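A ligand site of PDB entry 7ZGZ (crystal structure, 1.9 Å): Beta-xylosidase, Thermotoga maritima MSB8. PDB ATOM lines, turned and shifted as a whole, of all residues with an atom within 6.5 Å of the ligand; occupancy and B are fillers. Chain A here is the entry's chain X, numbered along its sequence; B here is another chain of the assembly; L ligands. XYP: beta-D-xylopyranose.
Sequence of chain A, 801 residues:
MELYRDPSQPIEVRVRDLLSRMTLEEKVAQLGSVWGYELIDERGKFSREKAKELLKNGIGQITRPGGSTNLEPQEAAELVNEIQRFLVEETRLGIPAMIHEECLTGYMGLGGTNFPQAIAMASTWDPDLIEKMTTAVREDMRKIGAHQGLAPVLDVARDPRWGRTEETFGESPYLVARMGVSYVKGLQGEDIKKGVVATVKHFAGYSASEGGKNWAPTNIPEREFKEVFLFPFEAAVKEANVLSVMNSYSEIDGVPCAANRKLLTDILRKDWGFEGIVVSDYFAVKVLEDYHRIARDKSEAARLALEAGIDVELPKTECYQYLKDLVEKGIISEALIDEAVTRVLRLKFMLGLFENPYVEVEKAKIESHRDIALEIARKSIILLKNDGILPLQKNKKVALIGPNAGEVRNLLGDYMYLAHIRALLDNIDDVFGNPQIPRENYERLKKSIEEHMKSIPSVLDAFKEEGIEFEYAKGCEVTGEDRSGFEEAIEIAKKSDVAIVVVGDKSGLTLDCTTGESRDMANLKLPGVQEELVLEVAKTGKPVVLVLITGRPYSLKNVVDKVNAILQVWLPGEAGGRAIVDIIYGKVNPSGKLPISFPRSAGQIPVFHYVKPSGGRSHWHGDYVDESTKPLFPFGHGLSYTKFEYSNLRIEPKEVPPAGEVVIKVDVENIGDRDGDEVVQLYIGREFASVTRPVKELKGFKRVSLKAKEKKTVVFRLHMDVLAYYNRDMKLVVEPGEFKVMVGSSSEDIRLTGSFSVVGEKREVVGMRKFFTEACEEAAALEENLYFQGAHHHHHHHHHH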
ATOM      1  N   ARG A  64       2.366 -19.090   7.680  1.00  0.00           N
ATOM      2  CA  ARG A  64       3.647 -19.419   8.367  1.00  0.00           C
ATOM      3  C   ARG A  64       3.554 -19.102   9.865  1.00  0.00           C
ATOM      4  O   ARG A  64       4.319 -18.289  10.380  1.00  0.00           O
ATOM      5  CB  ARG A  64       4.796 -18.638   7.708  1.00  0.00           C
ATOM      6  CG  ARG A  64       5.106 -19.029   6.268  1.00  0.00           C
ATOM      7  CD  ARG A  64       6.311 -18.223   5.772  1.00  0.00           C
ATOM      8  NE  ARG A  64       6.574 -18.329   4.351  1.00  0.00           N
ATOM      9  CZ  ARG A  64       7.607 -17.766   3.716  1.00  0.00           C
ATOM     10  NH1 ARG A  64       8.493 -17.033   4.378  1.00  0.00           N
ATOM     11  NH2 ARG A  64       7.746 -17.951   2.421  1.00  0.00           N
ATOM     12  N   GLU A 102       6.167 -22.999   4.388  1.00  0.00           N
ATOM     13  CA  GLU A 102       7.129 -23.511   3.379  1.00  0.00           C
ATOM     14  C   GLU A 102       7.586 -24.884   3.855  1.00  0.00           C
ATOM     15  O   GLU A 102       7.653 -25.090   5.069  1.00  0.00           O
ATOM     16  CB  GLU A 102       8.320 -22.543   3.235  1.00  0.00           C
ATOM     17  CG  GLU A 102       7.911 -21.141   2.819  1.00  0.00           C
ATOM     18  CD  GLU A 102       7.549 -21.008   1.352  1.00  0.00           C
ATOM     19  OE1 GLU A 102       7.795 -21.970   0.593  1.00  0.00           O
ATOM     20  OE2 GLU A 102       7.044 -19.944   0.961  1.00  0.00           O
ATOM     21  N   LEU A 150       3.954 -25.242   0.732  1.00  0.00           N
ATOM     22  CA  LEU A 150       4.153 -24.516  -0.560  1.00  0.00           C
ATOM     23  C   LEU A 150       5.277 -25.239  -1.318  1.00  0.00           C
ATOM     24  O   LEU A 150       6.305 -24.639  -1.570  1.00  0.00           O
ATOM     25  CB  LEU A 150       4.449 -23.046  -0.278  1.00  0.00           C
ATOM     26  CG  LEU A 150       3.380 -22.311   0.533  1.00  0.00           C
ATOM     27  CD1 LEU A 150       3.706 -20.821   0.626  1.00  0.00           C
ATOM     28  CD2 LEU A 150       1.995 -22.527  -0.052  1.00  0.00           C
ATOM     29  N   VAL A 153       8.327 -27.307  -6.403  1.00  0.00           N
ATOM     30  CA  VAL A 153       8.584 -26.453  -7.583  1.00  0.00           C
ATOM     31  C   VAL A 153       8.658 -27.392  -8.792  1.00  0.00           C
ATOM     32  O   VAL A 153       9.552 -28.229  -8.826  1.00  0.00           O
ATOM     33  CB  VAL A 153       9.864 -25.624  -7.387  1.00  0.00           C
ATOM     34  CG1 VAL A 153      10.250 -24.885  -8.664  1.00  0.00           C
ATOM     35  CG2 VAL A 153       9.729 -24.664  -6.204  1.00  0.00           C
ATOM     36  N   ARG A 164      16.941 -19.497  -8.790  1.00  0.00           N
ATOM     37  CA  ARG A 164      16.052 -20.531  -8.188  1.00  0.00           C
ATOM     38  C   ARG A 164      16.267 -21.893  -8.847  1.00  0.00           C
ATOM     39  O   ARG A 164      15.481 -22.800  -8.535  1.00  0.00           O
ATOM     40  CB  ARG A 164      14.599 -20.065  -8.251  1.00  0.00           C
ATOM     41  CG  ARG A 164      14.398 -18.742  -7.540  1.00  0.00           C
ATOM     42  CD  ARG A 164      12.944 -18.400  -7.357  1.00  0.00           C
ATOM     43  NE  ARG A 164      12.365 -19.136  -6.249  1.00  0.00           N
ATOM     44  CZ  ARG A 164      11.227 -18.830  -5.669  1.00  0.00           C
ATOM     45  NH1 ARG A 164      10.518 -17.807  -6.105  1.00  0.00           N
ATOM     46  NH2 ARG A 164      10.795 -19.552  -4.646  1.00  0.00           N
ATOM     47  N   GLU A 167      15.956 -24.900  -6.581  1.00  0.00           N
ATOM     48  CA  GLU A 167      14.591 -25.266  -6.106  1.00  0.00           C
ATOM     49  C   GLU A 167      13.873 -26.170  -7.113  1.00  0.00           C
ATOM     50  O   GLU A 167      12.796 -26.679  -6.792  1.00  0.00           O
ATOM     51  CB  GLU A 167      13.750 -24.016  -5.874  1.00  0.00           C
ATOM     52  CG  GLU A 167      14.260 -23.155  -4.742  1.00  0.00           C
ATOM     53  CD  GLU A 167      13.403 -21.936  -4.507  1.00  0.00           C
ATOM     54  OE1 GLU A 167      12.184 -22.105  -4.368  1.00  0.00           O
ATOM     55  OE2 GLU A 167      13.942 -20.819  -4.588  1.00  0.00           O
ATOM     56  N   LYS A 201       4.185 -25.231  -7.835  1.00  0.00           N
ATOM     57  CA  LYS A 201       4.523 -23.854  -8.242  1.00  0.00           C
ATOM     58  C   LYS A 201       5.664 -23.898  -9.260  1.00  0.00           C
ATOM     59  O   LYS A 201       6.385 -24.890  -9.309  1.00  0.00           O
ATOM     60  CB  LYS A 201       4.863 -23.055  -6.986  1.00  0.00           C
ATOM     61  CG  LYS A 201       6.045 -23.544  -6.150  1.00  0.00           C
ATOM     62  CD  LYS A 201       6.020 -22.977  -4.717  1.00  0.00           C
ATOM     63  CE  LYS A 201       7.377 -22.995  -4.039  1.00  0.00           C
ATOM     64  NZ  LYS A 201       7.332 -22.321  -2.717  1.00  0.00           N
ATOM     65  N   HIS A 202       5.850 -22.838 -10.055  1.00  0.00           N
ATOM     66  CA  HIS A 202       5.069 -21.613 -10.097  1.00  0.00           C
ATOM     67  C   HIS A 202       4.369 -21.545 -11.457  1.00  0.00           C
ATOM     68  O   HIS A 202       5.043 -21.352 -12.474  1.00  0.00           O
ATOM     69  CB  HIS A 202       5.982 -20.395  -9.859  1.00  0.00           C
ATOM     70  CG  HIS A 202       6.809 -20.489  -8.621  1.00  0.00           C
ATOM     71  ND1 HIS A 202       8.012 -21.184  -8.582  1.00  0.00           N
ATOM     72  CD2 HIS A 202       6.631 -19.966  -7.370  1.00  0.00           C
ATOM     73  CE1 HIS A 202       8.525 -21.098  -7.359  1.00  0.00           C
ATOM     74  NE2 HIS A 202       7.691 -20.363  -6.597  1.00  0.00           N
ATOM     75  N   TYR A 206       7.937 -19.882 -15.084  1.00  0.00           N
ATOM     76  CA  TYR A 206       8.696 -18.956 -14.205  1.00  0.00           C
ATOM     77  C   TYR A 206      10.218 -19.180 -14.267  1.00  0.00           C
ATOM     78  O   TYR A 206      10.908 -18.220 -14.015  1.00  0.00           O
ATOM     79  CB  TYR A 206       8.134 -19.084 -12.787  1.00  0.00           C
ATOM     80  CG  TYR A 206       8.809 -18.286 -11.705  1.00  0.00           C
ATOM     81  CD1 TYR A 206       8.941 -16.908 -11.782  1.00  0.00           C
ATOM     82  CD2 TYR A 206       9.204 -18.912 -10.525  1.00  0.00           C
ATOM     83  CE1 TYR A 206       9.531 -16.184 -10.746  1.00  0.00           C
ATOM     84  CE2 TYR A 206       9.763 -18.203  -9.481  1.00  0.00           C
ATOM     85  CZ  TYR A 206       9.944 -16.835  -9.597  1.00  0.00           C
ATOM     86  OH  TYR A 206      10.530 -16.150  -8.582  1.00  0.00           O
ATOM     87  N   TRP A 215      11.464 -12.784 -12.147  1.00  0.00           N
ATOM     88  CA  TRP A 215      10.168 -12.101 -12.500  1.00  0.00           C
ATOM     89  C   TRP A 215      10.131 -11.556 -13.948  1.00  0.00           C
ATOM     90  O   TRP A 215       9.107 -10.962 -14.294  1.00  0.00           O
ATOM     91  CB  TRP A 215       9.811 -10.958 -11.560  1.00  0.00           C
ATOM     92  CG  TRP A 215       9.553 -11.318 -10.121  1.00  0.00           C
ATOM     93  CD1 TRP A 215      10.121 -12.305  -9.380  1.00  0.00           C
ATOM     94  CD2 TRP A 215       8.713 -10.570  -9.228  1.00  0.00           C
ATOM     95  NE1 TRP A 215       9.656 -12.251  -8.088  1.00  0.00           N
ATOM     96  CE2 TRP A 215       8.795 -11.193  -7.969  1.00  0.00           C
ATOM     97  CE3 TRP A 215       7.874  -9.456  -9.396  1.00  0.00           C
ATOM     98  CZ2 TRP A 215       8.058 -10.738  -6.880  1.00  0.00           C
ATOM     99  CZ3 TRP A 215       7.142  -9.009  -8.310  1.00  0.00           C
ATOM    100  CH2 TRP A 215       7.263  -9.629  -7.075  1.00  0.00           C
ATOM    101  N   MET A 246       0.092 -22.711  -7.125  1.00  0.00           N
ATOM    102  CA  MET A 246       0.485 -21.296  -6.951  1.00  0.00           C
ATOM    103  C   MET A 246       0.918 -20.746  -8.313  1.00  0.00           C
ATOM    104  O   MET A 246       1.666 -21.433  -9.024  1.00  0.00           O
ATOM    105  CB  MET A 246       1.646 -21.185  -5.968  1.00  0.00           C
ATOM    106  CG  MET A 246       2.165 -19.769  -5.811  1.00  0.00           C
ATOM    107  SD  MET A 246       3.578 -19.666  -4.672  1.00  0.00           S
ATOM    108  CE  MET A 246       2.705 -19.681  -3.107  1.00  0.00           C
ATOM    109  N   TYR A 249       5.017 -15.306 -10.946  1.00  0.00           N
ATOM    110  CA  TYR A 249       5.155 -13.828 -10.868  1.00  0.00           C
ATOM    111  C   TYR A 249       5.296 -13.230 -12.272  1.00  0.00           C
ATOM    112  O   TYR A 249       5.044 -12.045 -12.453  1.00  0.00           O
ATOM    113  CB  TYR A 249       6.388 -13.469 -10.052  1.00  0.00           C
ATOM    114  CG  TYR A 249       6.248 -13.485  -8.550  1.00  0.00           C
ATOM    115  CD1 TYR A 249       5.268 -12.755  -7.892  1.00  0.00           C
ATOM    116  CD2 TYR A 249       7.175 -14.166  -7.778  1.00  0.00           C
ATOM    117  CE1 TYR A 249       5.199 -12.717  -6.506  1.00  0.00           C
ATOM    118  CE2 TYR A 249       7.128 -14.132  -6.389  1.00  0.00           C
ATOM    119  CZ  TYR A 249       6.150 -13.380  -5.754  1.00  0.00           C
ATOM    120  OH  TYR A 249       6.112 -13.392  -4.387  1.00  0.00           O
ATOM    121  N   ASP A 281       1.104 -16.494  -5.445  1.00  0.00           N
ATOM    122  CA  ASP A 281       2.463 -16.248  -4.931  1.00  0.00           C
ATOM    123  C   ASP A 281       2.356 -14.962  -4.092  1.00  0.00           C
ATOM    124  O   ASP A 281       1.358 -14.197  -4.266  1.00  0.00           O
ATOM    125  CB  ASP A 281       3.495 -16.187  -6.059  1.00  0.00           C
ATOM    126  CG  ASP A 281       4.891 -16.564  -5.564  1.00  0.00           C
ATOM    127  OD1 ASP A 281       5.103 -16.447  -4.349  1.00  0.00           O
ATOM    128  OD2 ASP A 281       5.723 -17.028  -6.396  1.00  0.00           O
ATOM    129  N   TYR A 282       3.300 -14.759  -3.180  1.00  0.00           N
ATOM    130  CA  TYR A 282       3.214 -13.693  -2.149  1.00  0.00           C
ATOM    131  C   TYR A 282       3.193 -12.327  -2.827  1.00  0.00           C
ATOM    132  O   TYR A 282       4.159 -12.003  -3.563  1.00  0.00           O
ATOM    133  CB  TYR A 282       4.375 -13.835  -1.168  1.00  0.00           C
ATOM    134  CG  TYR A 282       4.228 -14.907  -0.107  1.00  0.00           C
ATOM    135  CD1 TYR A 282       3.357 -15.982  -0.230  1.00  0.00           C
ATOM    136  CD2 TYR A 282       5.028 -14.859   1.014  1.00  0.00           C
ATOM    137  CE1 TYR A 282       3.266 -16.955   0.757  1.00  0.00           C
ATOM    138  CE2 TYR A 282       4.984 -15.831   1.988  1.00  0.00           C
ATOM    139  CZ  TYR A 282       4.103 -16.880   1.876  1.00  0.00           C
ATOM    140  OH  TYR A 282       4.098 -17.791   2.880  1.00  0.00           O
ATOM    141  N   PHE A 283       2.118 -11.575  -2.625  1.00  0.00           N
ATOM    142  CA  PHE A 283       1.931 -10.199  -3.152  1.00  0.00           C
ATOM    143  C   PHE A 283       1.707 -10.214  -4.685  1.00  0.00           C
ATOM    144  O   PHE A 283       1.713  -9.127  -5.302  1.00  0.00           O
ATOM    145  CB  PHE A 283       3.139  -9.312  -2.830  1.00  0.00           C
ATOM    146  CG  PHE A 283       3.665  -9.383  -1.409  1.00  0.00           C
ATOM    147  CD1 PHE A 283       2.948  -8.807  -0.369  1.00  0.00           C
ATOM    148  CD2 PHE A 283       4.851 -10.030  -1.110  1.00  0.00           C
ATOM    149  CE1 PHE A 283       3.419  -8.872   0.928  1.00  0.00           C
ATOM    150  CE2 PHE A 283       5.312 -10.116   0.197  1.00  0.00           C
ATOM    151  CZ  PHE A 283       4.601  -9.527   1.211  1.00  0.00           C
ATOM    152  N   TYR A 415      15.397 -21.980   1.101  1.00  0.00           N
ATOM    153  CA  TYR A 415      14.140 -22.267   1.857  1.00  0.00           C
ATOM    154  C   TYR A 415      14.425 -23.222   3.030  1.00  0.00           C
ATOM    155  O   TYR A 415      13.486 -23.801   3.598  1.00  0.00           O
ATOM    156  CB  TYR A 415      13.047 -22.735   0.881  1.00  0.00           C
ATOM    157  CG  TYR A 415      12.339 -21.559   0.272  1.00  0.00           C
ATOM    158  CD1 TYR A 415      12.871 -20.903  -0.830  1.00  0.00           C
ATOM    159  CD2 TYR A 415      11.248 -20.986   0.894  1.00  0.00           C
ATOM    160  CE1 TYR A 415      12.270 -19.755  -1.350  1.00  0.00           C
ATOM    161  CE2 TYR A 415      10.639 -19.839   0.395  1.00  0.00           C
ATOM    162  CZ  TYR A 415      11.157 -19.224  -0.731  1.00  0.00           C
ATOM    163  OH  TYR A 415      10.557 -18.092  -1.213  1.00  0.00           O
ATOM    164  N   HIS A 420      17.024 -18.876   5.376  1.00  0.00           N
ATOM    165  CA  HIS A 420      15.902 -18.000   4.920  1.00  0.00           C
ATOM    166  C   HIS A 420      15.636 -16.883   5.959  1.00  0.00           C
ATOM    167  O   HIS A 420      15.282 -15.783   5.517  1.00  0.00           O
ATOM    168  CB  HIS A 420      14.651 -18.844   4.564  1.00  0.00           C
ATOM    169  CG  HIS A 420      13.546 -18.097   3.877  1.00  0.00           C
ATOM    170  ND1 HIS A 420      13.301 -18.211   2.507  1.00  0.00           N
ATOM    171  CD2 HIS A 420      12.610 -17.237   4.347  1.00  0.00           C
ATOM    172  CE1 HIS A 420      12.284 -17.444   2.169  1.00  0.00           C
ATOM    173  NE2 HIS A 420      11.838 -16.837   3.287  1.00  0.00           N
ATOM    174  N   LEU A 509      18.421 -14.866   0.023  1.00  0.00           N
ATOM    175  CA  LEU A 509      17.533 -13.846  -0.580  1.00  0.00           C
ATOM    176  C   LEU A 509      18.169 -12.461  -0.515  1.00  0.00           C
ATOM    177  O   LEU A 509      17.580 -11.540  -1.089  1.00  0.00           O
ATOM    178  CB  LEU A 509      16.176 -13.889   0.128  1.00  0.00           C
ATOM    179  CG  LEU A 509      15.136 -14.771  -0.576  1.00  0.00           C
ATOM    180  CD1 LEU A 509      15.606 -16.218  -0.637  1.00  0.00           C
ATOM    181  CD2 LEU A 509      13.782 -14.681   0.120  1.00  0.00           C
ATOM    182  N   GLU A 517      16.599 -17.358  -4.639  1.00  0.00           N
ATOM    183  CA  GLU A 517      15.577 -16.391  -5.106  1.00  0.00           C
ATOM    184  C   GLU A 517      16.158 -14.959  -5.041  1.00  0.00           C
ATOM    185  O   GLU A 517      16.577 -14.549  -3.940  1.00  0.00           O
ATOM    186  CB  GLU A 517      14.343 -16.530  -4.212  1.00  0.00           C
ATOM    187  CG  GLU A 517      13.219 -15.597  -4.582  1.00  0.00           C
ATOM    188  CD  GLU A 517      12.001 -15.830  -3.698  1.00  0.00           C
ATOM    189  OE1 GLU A 517      12.078 -16.712  -2.822  1.00  0.00           O
ATOM    190  OE2 GLU A 517      11.009 -15.115  -3.885  1.00  0.00           O
ATOM    191  N   TRP B 620      14.451  -8.535  -6.906  1.00  0.00           N
ATOM    192  CA  TRP B 620      14.030  -7.251  -6.288  1.00  0.00           C
ATOM    193  C   TRP B 620      15.321  -6.449  -6.013  1.00  0.00           C
ATOM    194  O   TRP B 620      15.176  -5.319  -5.534  1.00  0.00           O
ATOM    195  CB  TRP B 620      13.089  -7.354  -5.080  1.00  0.00           C
ATOM    196  CG  TRP B 620      13.605  -8.239  -3.991  1.00  0.00           C
ATOM    197  CD1 TRP B 620      14.505  -7.921  -3.009  1.00  0.00           C
ATOM    198  CD2 TRP B 620      13.270  -9.618  -3.802  1.00  0.00           C
ATOM    199  NE1 TRP B 620      14.727  -9.001  -2.211  1.00  0.00           N
ATOM    200  CE2 TRP B 620      13.997 -10.065  -2.673  1.00  0.00           C
ATOM    201  CE3 TRP B 620      12.413 -10.514  -4.460  1.00  0.00           C
ATOM    202  CZ2 TRP B 620      13.892 -11.374  -2.202  1.00  0.00           C
ATOM    203  CZ3 TRP B 620      12.312 -11.799  -3.987  1.00  0.00           C
ATOM    204  CH2 TRP B 620      13.046 -12.233  -2.884  1.00  0.00           C
HETATM  205  O1  XYP L   1       8.516 -15.020  -2.635  1.00  0.00           O
HETATM  206  C1  XYP L   1       7.572 -16.051  -2.798  1.00  0.00           C
HETATM  207  C2  XYP L   1       8.084 -17.318  -3.593  1.00  0.00           C
HETATM  208  C3  XYP L   1       7.247 -18.565  -3.348  1.00  0.00           C
HETATM  209  C4  XYP L   1       6.983 -18.749  -1.868  1.00  0.00           C
HETATM  210  C5  XYP L   1       6.369 -17.486  -1.304  1.00  0.00           C
HETATM  211  O2  XYP L   1       8.132 -17.142  -5.013  1.00  0.00           O
HETATM  212  O3  XYP L   1       7.945 -19.693  -3.848  1.00  0.00           O
HETATM  213  O4  XYP L   1       6.096 -19.855  -1.678  1.00  0.00           O
HETATM  214  O5  XYP L   1       7.279 -16.384  -1.433  1.00  0.00           O
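The side-chain hydroxyl (OH) of Tyr 249 sits at hydrogen-bond distance from the backbone carbonyl oxygen (O) of Tyr 282 (2.5 Å).
OE2 of Glu 167 is in salt-bridge range of NE of Arg 164, 2.8 Å away.
OE2 of Glu 102 lies within salt-bridge range of NH2 of Arg 64 (2.6 Å).
The guanidinium group (NH1) of Arg 164 sits at hydrogen-bond distance from the side-chain hydroxyl (OH) of Tyr 206.
OE1 of Glu 102 is in salt-bridge range of NZ of Lys 201 (3.4 Å).
NZ of Lys 201 is in hydrogen-bond range of O of Leu 150.
The guanidinium group (NH1) of Arg 164 lies within salt-bridge range of the side-chain carboxylate (OE2) of Glu 517.
OE1 of Glu 517 sits at hydrogen-bond distance from OH of Tyr 415, 2.6 Å away.
An oxygen (O3) of the ligand sits at hydrogen-bond distance from a ring nitrogen (NE2) of His 202 (2.8 Å).
The side-chain amino group of Lys 201 sits at hydrogen-bond distance from an oxygen (O3) of the ligand, 2.9 Å away.
O1 of the ligand is in hydrogen-bond range of OH of Tyr 249, at 3.4 Å.
OE2 of Glu 517 sits at hydrogen-bond distance from O1 of the ligand, 2.8 Å away.
The guanidinium group (NH1) of Arg 164 lies within hydrogen-bond range of an oxygen (O2) of the ligand (2.7 Å).
The side-chain carboxylate (OD2) of Asp 281 sits at hydrogen-bond distance from an oxygen (O2) of the ligand (2.8 Å).
The side-chain carboxylate (OE2) of Glu 102 lies within hydrogen-bond range of an oxygen (O4) of the ligand (2.8 Å).
Residues that only touch the ligand: Arg 64 (3.998 Å), Leu 150 (3.5 Å), Met 246 (3.7 Å), Tyr 282 (3.5 Å) and Tyr 415 (3.5 Å).
Hydrophobic or aromatic side chains within 4 Å of the ligand: Leu 150, His 202, Met 246, Tyr 249 and Tyr 282.
12 residues have an atom within 4 Å of the ligand: Arg 64, Glu 102, Leu 150, Arg 164, Lys 201, His 202, Met 246, Tyr 249, Asp 281, Tyr 282, Tyr 415 and Glu 517.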
